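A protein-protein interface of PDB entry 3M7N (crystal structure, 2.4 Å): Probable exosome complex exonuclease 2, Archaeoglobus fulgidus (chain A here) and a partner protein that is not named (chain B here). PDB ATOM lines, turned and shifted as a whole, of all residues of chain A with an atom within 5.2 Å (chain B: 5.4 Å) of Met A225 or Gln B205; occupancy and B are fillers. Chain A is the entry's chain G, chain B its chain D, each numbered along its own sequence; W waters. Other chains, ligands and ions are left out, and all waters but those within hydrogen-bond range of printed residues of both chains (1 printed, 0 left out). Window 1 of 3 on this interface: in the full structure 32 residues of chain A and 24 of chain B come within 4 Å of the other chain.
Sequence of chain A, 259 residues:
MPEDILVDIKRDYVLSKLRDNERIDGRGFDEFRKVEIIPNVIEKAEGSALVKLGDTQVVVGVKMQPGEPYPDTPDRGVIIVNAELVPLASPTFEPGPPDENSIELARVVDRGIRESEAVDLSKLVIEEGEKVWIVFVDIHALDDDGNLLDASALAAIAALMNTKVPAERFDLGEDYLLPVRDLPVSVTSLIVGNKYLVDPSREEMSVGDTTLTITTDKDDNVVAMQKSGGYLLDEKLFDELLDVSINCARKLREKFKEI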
ATOM      1  N   ARG A 111      13.897  23.027  -8.038  1.00  0.00           N
ATOM      2  CA  ARG A 111      13.545  23.758  -9.261  1.00  0.00           C
ATOM      3  C   ARG A 111      14.163  25.153  -9.312  1.00  0.00           C
ATOM      4  O   ARG A 111      14.770  25.537 -10.325  1.00  0.00           O
ATOM      5  CB  ARG A 111      12.026  23.829  -9.433  1.00  0.00           C
ATOM      6  CG  ARG A 111      11.438  22.534  -9.969  1.00  0.00           C
ATOM      7  CD  ARG A 111      10.068  22.271  -9.397  1.00  0.00           C
ATOM      8  NE  ARG A 111       9.080  23.211  -9.884  1.00  0.00           N
ATOM      9  CZ  ARG A 111       7.900  23.382  -9.314  1.00  0.00           C
ATOM     10  NH1 ARG A 111       7.028  24.255  -9.807  1.00  0.00           N
ATOM     11  NH2 ARG A 111       7.589  22.668  -8.252  1.00  0.00           N
ATOM     12  N   LEU A 212       0.954  29.999  -2.203  1.00  0.00           N
ATOM     13  CA  LEU A 212       1.500  30.255  -3.530  1.00  0.00           C
ATOM     14  C   LEU A 212       2.971  30.530  -3.312  1.00  0.00           C
ATOM     15  O   LEU A 212       3.351  31.176  -2.343  1.00  0.00           O
ATOM     16  CB  LEU A 212       0.837  31.485  -4.163  1.00  0.00           C
ATOM     17  CG  LEU A 212       0.813  31.760  -5.681  1.00  0.00           C
ATOM     18  CD1 LEU A 212       1.326  33.161  -5.985  1.00  0.00           C
ATOM     19  CD2 LEU A 212       1.552  30.728  -6.534  1.00  0.00           C
ATOM     20  N   THR A 213       3.809  30.038  -4.206  1.00  0.00           N
ATOM     21  CA  THR A 213       5.229  30.243  -4.044  1.00  0.00           C
ATOM     22  C   THR A 213       5.844  30.679  -5.363  1.00  0.00           C
ATOM     23  O   THR A 213       5.592  30.072  -6.415  1.00  0.00           O
ATOM     24  CB  THR A 213       5.906  28.957  -3.543  1.00  0.00           C
ATOM     25  OG1 THR A 213       5.393  28.625  -2.243  1.00  0.00           O
ATOM     26  CG2 THR A 213       7.411  29.129  -3.480  1.00  0.00           C
ATOM     27  N   ILE A 214       6.653  31.733  -5.299  1.00  0.00           N
ATOM     28  CA  ILE A 214       7.311  32.290  -6.472  1.00  0.00           C
ATOM     29  C   ILE A 214       8.789  32.375  -6.190  1.00  0.00           C
ATOM     30  O   ILE A 214       9.189  32.796  -5.115  1.00  0.00           O
ATOM     31  CB  ILE A 214       6.789  33.704  -6.793  1.00  0.00           C
ATOM     32  CG1 ILE A 214       5.278  33.661  -7.048  1.00  0.00           C
ATOM     33  CG2 ILE A 214       7.553  34.308  -7.976  1.00  0.00           C
ATOM     34  CD1 ILE A 214       4.658  34.996  -7.300  1.00  0.00           C
ATOM     35  N   THR A 215       9.595  31.985  -7.164  1.00  0.00           N
ATOM     36  CA  THR A 215      11.021  31.917  -6.987  1.00  0.00           C
ATOM     37  C   THR A 215      11.715  32.679  -8.113  1.00  0.00           C
ATOM     38  O   THR A 215      11.518  32.376  -9.298  1.00  0.00           O
ATOM     39  CB  THR A 215      11.510  30.441  -6.948  1.00  0.00           C
ATOM     40  OG1 THR A 215      10.804  29.726  -5.926  1.00  0.00           O
ATOM     41  CG2 THR A 215      12.991  30.374  -6.664  1.00  0.00           C
ATOM     42  N   VAL A 222      11.410  35.368 -12.956  1.00  0.00           N
ATOM     43  CA  VAL A 222      10.773  34.247 -12.298  1.00  0.00           C
ATOM     44  C   VAL A 222      11.336  32.947 -12.855  1.00  0.00           C
ATOM     45  O   VAL A 222      11.488  32.779 -14.067  1.00  0.00           O
ATOM     46  CB  VAL A 222       9.264  34.297 -12.431  1.00  0.00           C
ATOM     47  CG1 VAL A 222       8.666  33.047 -11.832  1.00  0.00           C
ATOM     48  CG2 VAL A 222       8.727  35.535 -11.723  1.00  0.00           C
ATOM     49  N   VAL A 223      11.687  32.039 -11.953  1.00  0.00           N
ATOM     50  CA  VAL A 223      12.402  30.841 -12.356  1.00  0.00           C
ATOM     51  C   VAL A 223      11.617  29.574 -12.009  1.00  0.00           C
ATOM     52  O   VAL A 223      11.856  28.500 -12.569  1.00  0.00           O
ATOM     53  CB  VAL A 223      13.845  30.869 -11.794  1.00  0.00           C
ATOM     54  CG1 VAL A 223      14.299  29.517 -11.279  1.00  0.00           C
ATOM     55  CG2 VAL A 223      14.799  31.389 -12.855  1.00  0.00           C
ATOM     56  N   ALA A 224      10.652  29.720 -11.109  1.00  0.00           N
ATOM     57  CA  ALA A 224       9.774  28.625 -10.745  1.00  0.00           C
ATOM     58  C   ALA A 224       8.607  29.169  -9.932  1.00  0.00           C
ATOM     59  O   ALA A 224       8.751  30.175  -9.241  1.00  0.00           O
ATOM     60  CB  ALA A 224      10.543  27.569  -9.948  1.00  0.00           C
ATOM     61  N   MET A 225       7.443  28.532 -10.052  1.00  0.00           N
ATOM     62  CA  MET A 225       6.303  28.886  -9.221  1.00  0.00           C
ATOM     63  C   MET A 225       5.555  27.615  -8.857  1.00  0.00           C
ATOM     64  O   MET A 225       5.746  26.576  -9.501  1.00  0.00           O
ATOM     65  CB  MET A 225       5.344  29.814  -9.958  1.00  0.00           C
ATOM     66  CG  MET A 225       5.994  30.862 -10.840  1.00  0.00           C
ATOM     67  SD  MET A 225       4.768  32.061 -11.413  1.00  0.00           S
ATOM     68  CE  MET A 225       4.180  32.701  -9.861  1.00  0.00           C
ATOM     69  N   GLN A 226       4.679  27.718  -7.856  1.00  0.00           N
ATOM     70  CA  GLN A 226       3.905  26.581  -7.384  1.00  0.00           C
ATOM     71  C   GLN A 226       2.727  27.022  -6.521  1.00  0.00           C
ATOM     72  O   GLN A 226       2.910  27.518  -5.412  1.00  0.00           O
ATOM     73  CB  GLN A 226       4.802  25.646  -6.563  1.00  0.00           C
ATOM     74  CG  GLN A 226       4.122  24.396  -6.073  1.00  0.00           C
ATOM     75  CD  GLN A 226       3.995  23.363  -7.165  1.00  0.00           C
ATOM     76  OE1 GLN A 226       4.894  23.204  -8.000  1.00  0.00           O
ATOM     77  NE2 GLN A 226       2.872  22.657  -7.176  1.00  0.00           N
ATOM     78  N   LYS A 227       1.518  26.838  -7.034  1.00  0.00           N
ATOM     79  CA  LYS A 227       0.314  27.021  -6.245  1.00  0.00           C
ATOM     80  C   LYS A 227       0.007  25.690  -5.532  1.00  0.00           C
ATOM     81  O   LYS A 227       0.195  24.626  -6.127  1.00  0.00           O
ATOM     82  CB  LYS A 227      -0.842  27.416  -7.171  1.00  0.00           C
ATOM     83  CG  LYS A 227      -2.204  27.471  -6.488  1.00  0.00           C
ATOM     84  CD  LYS A 227      -3.342  27.716  -7.494  1.00  0.00           C
ATOM     85  CE  LYS A 227      -4.714  27.660  -6.817  1.00  0.00           C
ATOM     86  NZ  LYS A 227      -5.140  26.269  -6.522  1.00  0.00           N
ATOM     87  N   PHE A 238      -3.072  37.349  -8.131  1.00  0.00           N
ATOM     88  CA  PHE A 238      -1.830  36.807  -8.642  1.00  0.00           C
ATOM     89  C   PHE A 238      -0.929  37.904  -9.189  1.00  0.00           C
ATOM     90  O   PHE A 238       0.246  37.980  -8.832  1.00  0.00           O
ATOM     91  CB  PHE A 238      -2.056  35.744  -9.713  1.00  0.00           C
ATOM     92  CG  PHE A 238      -0.779  35.190 -10.262  1.00  0.00           C
ATOM     93  CD1 PHE A 238      -0.098  34.193  -9.585  1.00  0.00           C
ATOM     94  CD2 PHE A 238      -0.235  35.694 -11.421  1.00  0.00           C
ATOM     95  CE1 PHE A 238       1.093  33.682 -10.077  1.00  0.00           C
ATOM     96  CE2 PHE A 238       0.955  35.192 -11.919  1.00  0.00           C
ATOM     97  CZ  PHE A 238       1.621  34.178 -11.245  1.00  0.00           C
ATOM     98  N   LEU A 242       2.690  38.796  -7.703  1.00  0.00           N
ATOM     99  CA  LEU A 242       3.872  38.579  -8.530  1.00  0.00           C
ATOM    100  C   LEU A 242       4.926  39.649  -8.238  1.00  0.00           C
ATOM    101  O   LEU A 242       6.108  39.340  -7.988  1.00  0.00           O
ATOM    102  CB  LEU A 242       3.510  38.601 -10.016  1.00  0.00           C
ATOM    103  CG  LEU A 242       4.351  37.725 -10.950  1.00  0.00           C
ATOM    104  CD1 LEU A 242       4.168  38.158 -12.399  1.00  0.00           C
ATOM    105  CD2 LEU A 242       5.822  37.740 -10.578  1.00  0.00           C
ATOM    106  N   GLU B 100       3.786  14.121  -6.883  1.00  0.00           N
ATOM    107  CA  GLU B 100       3.609  15.565  -6.938  1.00  0.00           C
ATOM    108  C   GLU B 100       2.417  15.913  -7.821  1.00  0.00           C
ATOM    109  O   GLU B 100       1.489  16.605  -7.390  1.00  0.00           O
ATOM    110  CB  GLU B 100       4.889  16.243  -7.429  1.00  0.00           C
ATOM    111  CG  GLU B 100       4.675  17.466  -8.298  1.00  0.00           C
ATOM    112  CD  GLU B 100       4.148  18.651  -7.521  1.00  0.00           C
ATOM    113  OE1 GLU B 100       4.607  18.858  -6.379  1.00  0.00           O
ATOM    114  OE2 GLU B 100       3.277  19.374  -8.048  1.00  0.00           O
ATOM    115  N   VAL B 104      -1.177  18.005  -6.616  1.00  0.00           N
ATOM    116  CA  VAL B 104      -1.648  19.273  -7.161  1.00  0.00           C
ATOM    117  C   VAL B 104      -2.913  19.071  -8.012  1.00  0.00           C
ATOM    118  O   VAL B 104      -3.809  19.927  -8.035  1.00  0.00           O
ATOM    119  CB  VAL B 104      -0.534  20.009  -7.950  1.00  0.00           C
ATOM    120  CG1 VAL B 104      -0.256  19.331  -9.286  1.00  0.00           C
ATOM    121  CG2 VAL B 104      -0.926  21.440  -8.155  1.00  0.00           C
ATOM    122  N   ARG B 137       0.055  15.782 -17.743  1.00  0.00           N
ATOM    123  CA  ARG B 137      -0.713  16.105 -16.533  1.00  0.00           C
ATOM    124  C   ARG B 137      -1.882  16.985 -16.923  1.00  0.00           C
ATOM    125  O   ARG B 137      -2.940  16.997 -16.292  1.00  0.00           O
ATOM    126  CB  ARG B 137       0.166  16.794 -15.472  1.00  0.00           C
ATOM    127  CG  ARG B 137       0.332  18.287 -15.637  1.00  0.00           C
ATOM    128  CD  ARG B 137       1.289  18.864 -14.595  1.00  0.00           C
ATOM    129  NE  ARG B 137       2.654  18.398 -14.813  1.00  0.00           N
ATOM    130  CZ  ARG B 137       3.678  18.638 -13.994  1.00  0.00           C
ATOM    131  NH1 ARG B 137       3.503  19.351 -12.892  1.00  0.00           N
ATOM    132  NH2 ARG B 137       4.883  18.152 -14.275  1.00  0.00           N
ATOM    133  N   ASP B 186       8.274  26.256 -19.025  1.00  0.00           N
ATOM    134  CA  ASP B 186       7.084  25.434 -19.177  1.00  0.00           C
ATOM    135  C   ASP B 186       6.154  25.696 -17.989  1.00  0.00           C
ATOM    136  O   ASP B 186       6.568  25.614 -16.835  1.00  0.00           O
ATOM    137  CB  ASP B 186       7.446  23.947 -19.266  1.00  0.00           C
ATOM    138  CG  ASP B 186       6.200  23.035 -19.355  1.00  0.00           C
ATOM    139  OD1 ASP B 186       6.289  21.864 -18.946  1.00  0.00           O
ATOM    140  OD2 ASP B 186       5.126  23.481 -19.818  1.00  0.00           O
ATOM    141  N   MET B 187       4.898  26.011 -18.268  1.00  0.00           N
ATOM    142  CA  MET B 187       3.982  26.459 -17.234  1.00  0.00           C
ATOM    143  C   MET B 187       2.560  25.876 -17.398  1.00  0.00           C
ATOM    144  O   MET B 187       1.747  26.414 -18.158  1.00  0.00           O
ATOM    145  CB  MET B 187       3.946  27.981 -17.276  1.00  0.00           C
ATOM    146  CG  MET B 187       3.149  28.652 -16.175  1.00  0.00           C
ATOM    147  SD  MET B 187       3.530  30.425 -16.156  1.00  0.00           S
ATOM    148  CE  MET B 187       2.312  30.982 -14.972  1.00  0.00           C
ATOM    149  N   PRO B 188       2.258  24.770 -16.680  1.00  0.00           N
ATOM    150  CA  PRO B 188       0.913  24.163 -16.629  1.00  0.00           C
ATOM    151  C   PRO B 188      -0.093  25.083 -15.972  1.00  0.00           C
ATOM    152  O   PRO B 188       0.254  25.671 -14.951  1.00  0.00           O
ATOM    153  CB  PRO B 188       1.102  22.964 -15.695  1.00  0.00           C
ATOM    154  CG  PRO B 188       2.573  22.699 -15.667  1.00  0.00           C
ATOM    155  CD  PRO B 188       3.242  24.009 -15.885  1.00  0.00           C
ATOM    156  N   LEU B 203      -4.949  25.606 -10.879  1.00  0.00           N
ATOM    157  CA  LEU B 203      -3.630  25.000 -10.872  1.00  0.00           C
ATOM    158  C   LEU B 203      -2.629  25.910 -11.547  1.00  0.00           C
ATOM    159  O   LEU B 203      -2.890  26.438 -12.625  1.00  0.00           O
ATOM    160  CB  LEU B 203      -3.646  23.633 -11.563  1.00  0.00           C
ATOM    161  CG  LEU B 203      -2.294  22.911 -11.643  1.00  0.00           C
ATOM    162  CD1 LEU B 203      -2.508  21.398 -11.582  1.00  0.00           C
ATOM    163  CD2 LEU B 203      -1.471  23.281 -12.874  1.00  0.00           C
ATOM    164  N   LEU B 204      -1.476  26.084 -10.912  1.00  0.00           N
ATOM    165  CA  LEU B 204      -0.428  26.902 -11.480  1.00  0.00           C
ATOM    166  C   LEU B 204       0.938  26.365 -11.060  1.00  0.00           C
ATOM    167  O   LEU B 204       1.215  26.209  -9.877  1.00  0.00           O
ATOM    168  CB  LEU B 204      -0.609  28.360 -11.037  1.00  0.00           C
ATOM    169  CG  LEU B 204       0.176  29.433 -11.791  1.00  0.00           C
ATOM    170  CD1 LEU B 204      -0.477  30.810 -11.633  1.00  0.00           C
ATOM    171  CD2 LEU B 204       1.607  29.456 -11.319  1.00  0.00           C
ATOM    172  N   GLN B 205       1.775  26.080 -12.048  1.00  0.00           N
ATOM    173  CA  GLN B 205       3.142  25.636 -11.825  1.00  0.00           C
ATOM    174  C   GLN B 205       4.008  26.215 -12.934  1.00  0.00           C
ATOM    175  O   GLN B 205       3.549  26.349 -14.071  1.00  0.00           O
ATOM    176  CB  GLN B 205       3.237  24.106 -11.884  1.00  0.00           C
ATOM    177  CG  GLN B 205       2.453  23.348 -10.830  1.00  0.00           C
ATOM    178  CD  GLN B 205       2.734  21.845 -10.888  1.00  0.00           C
ATOM    179  OE1 GLN B 205       2.188  21.124 -11.732  1.00  0.00           O
ATOM    180  NE2 GLN B 205       3.601  21.374  -9.997  1.00  0.00           N
ATOM    181  N   MET B 206       5.247  26.568 -12.619  1.00  0.00           N
ATOM    182  CA  MET B 206       6.186  26.963 -13.657  1.00  0.00           C
ATOM    183  C   MET B 206       7.594  26.538 -13.303  1.00  0.00           C
ATOM    184  O   MET B 206       8.010  26.616 -12.157  1.00  0.00           O
ATOM    185  CB  MET B 206       6.123  28.477 -13.952  1.00  0.00           C
ATOM    186  CG  MET B 206       7.238  29.332 -13.321  1.00  0.00           C
ATOM    187  SD  MET B 206       8.780  29.379 -14.262  1.00  0.00           S
ATOM    188  CE  MET B 206       8.881  31.084 -14.752  1.00  0.00           C
ATOM    189  N   ASP B 207       8.321  26.093 -14.313  1.00  0.00           N
ATOM    190  CA  ASP B 207       9.733  25.823 -14.189  1.00  0.00           C
ATOM    191  C   ASP B 207      10.397  26.545 -15.361  1.00  0.00           C
ATOM    192  O   ASP B 207       9.867  26.524 -16.471  1.00  0.00           O
ATOM    193  CB  ASP B 207       9.983  24.308 -14.253  1.00  0.00           C
ATOM    194  N   VAL B 215       5.353  36.194 -17.855  1.00  0.00           N
ATOM    195  CA  VAL B 215       4.442  35.414 -17.021  1.00  0.00           C
ATOM    196  C   VAL B 215       2.994  35.847 -17.207  1.00  0.00           C
ATOM    197  O   VAL B 215       2.134  35.016 -17.479  1.00  0.00           O
ATOM    198  CB  VAL B 215       4.819  35.501 -15.531  1.00  0.00           C
ATOM    199  CG1 VAL B 215       3.828  34.743 -14.684  1.00  0.00           C
ATOM    200  CG2 VAL B 215       6.233  34.985 -15.318  1.00  0.00           C
HETATM  201  O   HOH W   1      -1.508  24.341  -8.472  1.00  0.00           O
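OE2 of Glu B100 is in hydrogen-bond range of NE2 of Gln A226, 3.4 Å away.
The backbone carbonyl oxygen of Leu B204 lies within hydrogen-bond range of the backbone NH of Lys A227, 2.9 Å away.
NE2 of Gln B205 sits at hydrogen-bond distance from OE1 of Gln A226.
The backbone carbonyl oxygen (O) of Met B206 is in hydrogen-bond range of the guanidinium group (NH1) of Arg A111 (3.5 Å).
SD of Met B206 is in hydrogen-bond range of N of Ala A224, 3.7 Å away.
O of Met B206 sits at hydrogen-bond distance from N of Met A225.
The backbone carbonyl oxygen (O) of Val A223 lies close to the side-chain sulfur (SD) of Met B206 (3.6 Å).
The side-chain carboxylate (OE2) of Glu B100 sits at hydrogen-bond distance from the side-chain amide nitrogen (NE2) of Gln B205, 2.8 Å away.
The side-chain amide oxygen (OE1) of Gln B205 lies within hydrogen-bond range of the guanidinium group (NH1) of Arg B137, 2.5 Å away.
O of Asp B207 sits at hydrogen-bond distance from N of Asp B186, 3.0 Å away.
O of Met A225 lies within hydrogen-bond range of NH1 of Arg A111, 2.7 Å away.
The guanidinium group (NH2) of Arg A111 is in hydrogen-bond range of the side-chain amide oxygen (OE1) of Gln A226.
The backbone carbonyl oxygen (O) of Thr A213 sits at hydrogen-bond distance from the backbone NH (N) of Gln A226 (2.9 Å).
Among the printed residues, pairs that only touch across the chains: Val A222 with Met B206 (3.2 Å), Met A225 with Gln B205 (3.6 Å), Phe A238 with Leu B204 (3.6 Å), Gln A226 with Leu B204 (3.7 Å), Val A223 with Asp B207 (3.7 Å), Lys A227 with Val B104 (3.9 Å) and Met A225 with Leu B204 (3.99 Å).
Gln B205 touches two residues of chain A.
Printed residues of chain A within 4 Å of Glu B100: Gln A226.
Of the printed residues of chain B, Gln A226 touches Glu B100 (3.4 Å), Leu B204 (3.7 Å) and Gln B205 (3.0 Å).
Printed residues of chain B within 4 Å of Phe A238: Leu B204.
Printed residues of chain B within 4 Å of Lys A227: Val B104 (3.9 Å) and Leu B204 (2.9 Å).
Leu A242 touches none of the printed residues of chain B.
Val B215 touches none of the printed residues of chain A.
The nearest printed residue of chain B that does not touch Met A225 is Val B215 (4.3 Å).
The nearest residue of chain A that does not touch Gln B205 is Arg A111 (4.3 Å).
The nearest printed residue of chain A that does not touch Glu B100 is Arg A111 (5.2 Å).
Printed residues of chain B that touch a printed residue of chain A: Glu B100, Val B104, Leu B204, Gln B205, Met B206 and Asp B207.
Hydrophobic or aromatic side chains of chain B that line the printed part of chain A: Val B104, Leu B204 and Met B206.
Along chain B the printed residues that touch a printed residue of chain A span positions 100 to 207.
Among the printed residues, 14 pairs touch across the chains.
Among the printed residues, no Asp or Glu carboxylate lies within 4 Å of a Lys or Arg side-chain nitrogen of the other chain.
Water W1 lies within hydrogen-bond range of O of Lys A227 and N of Leu B204.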
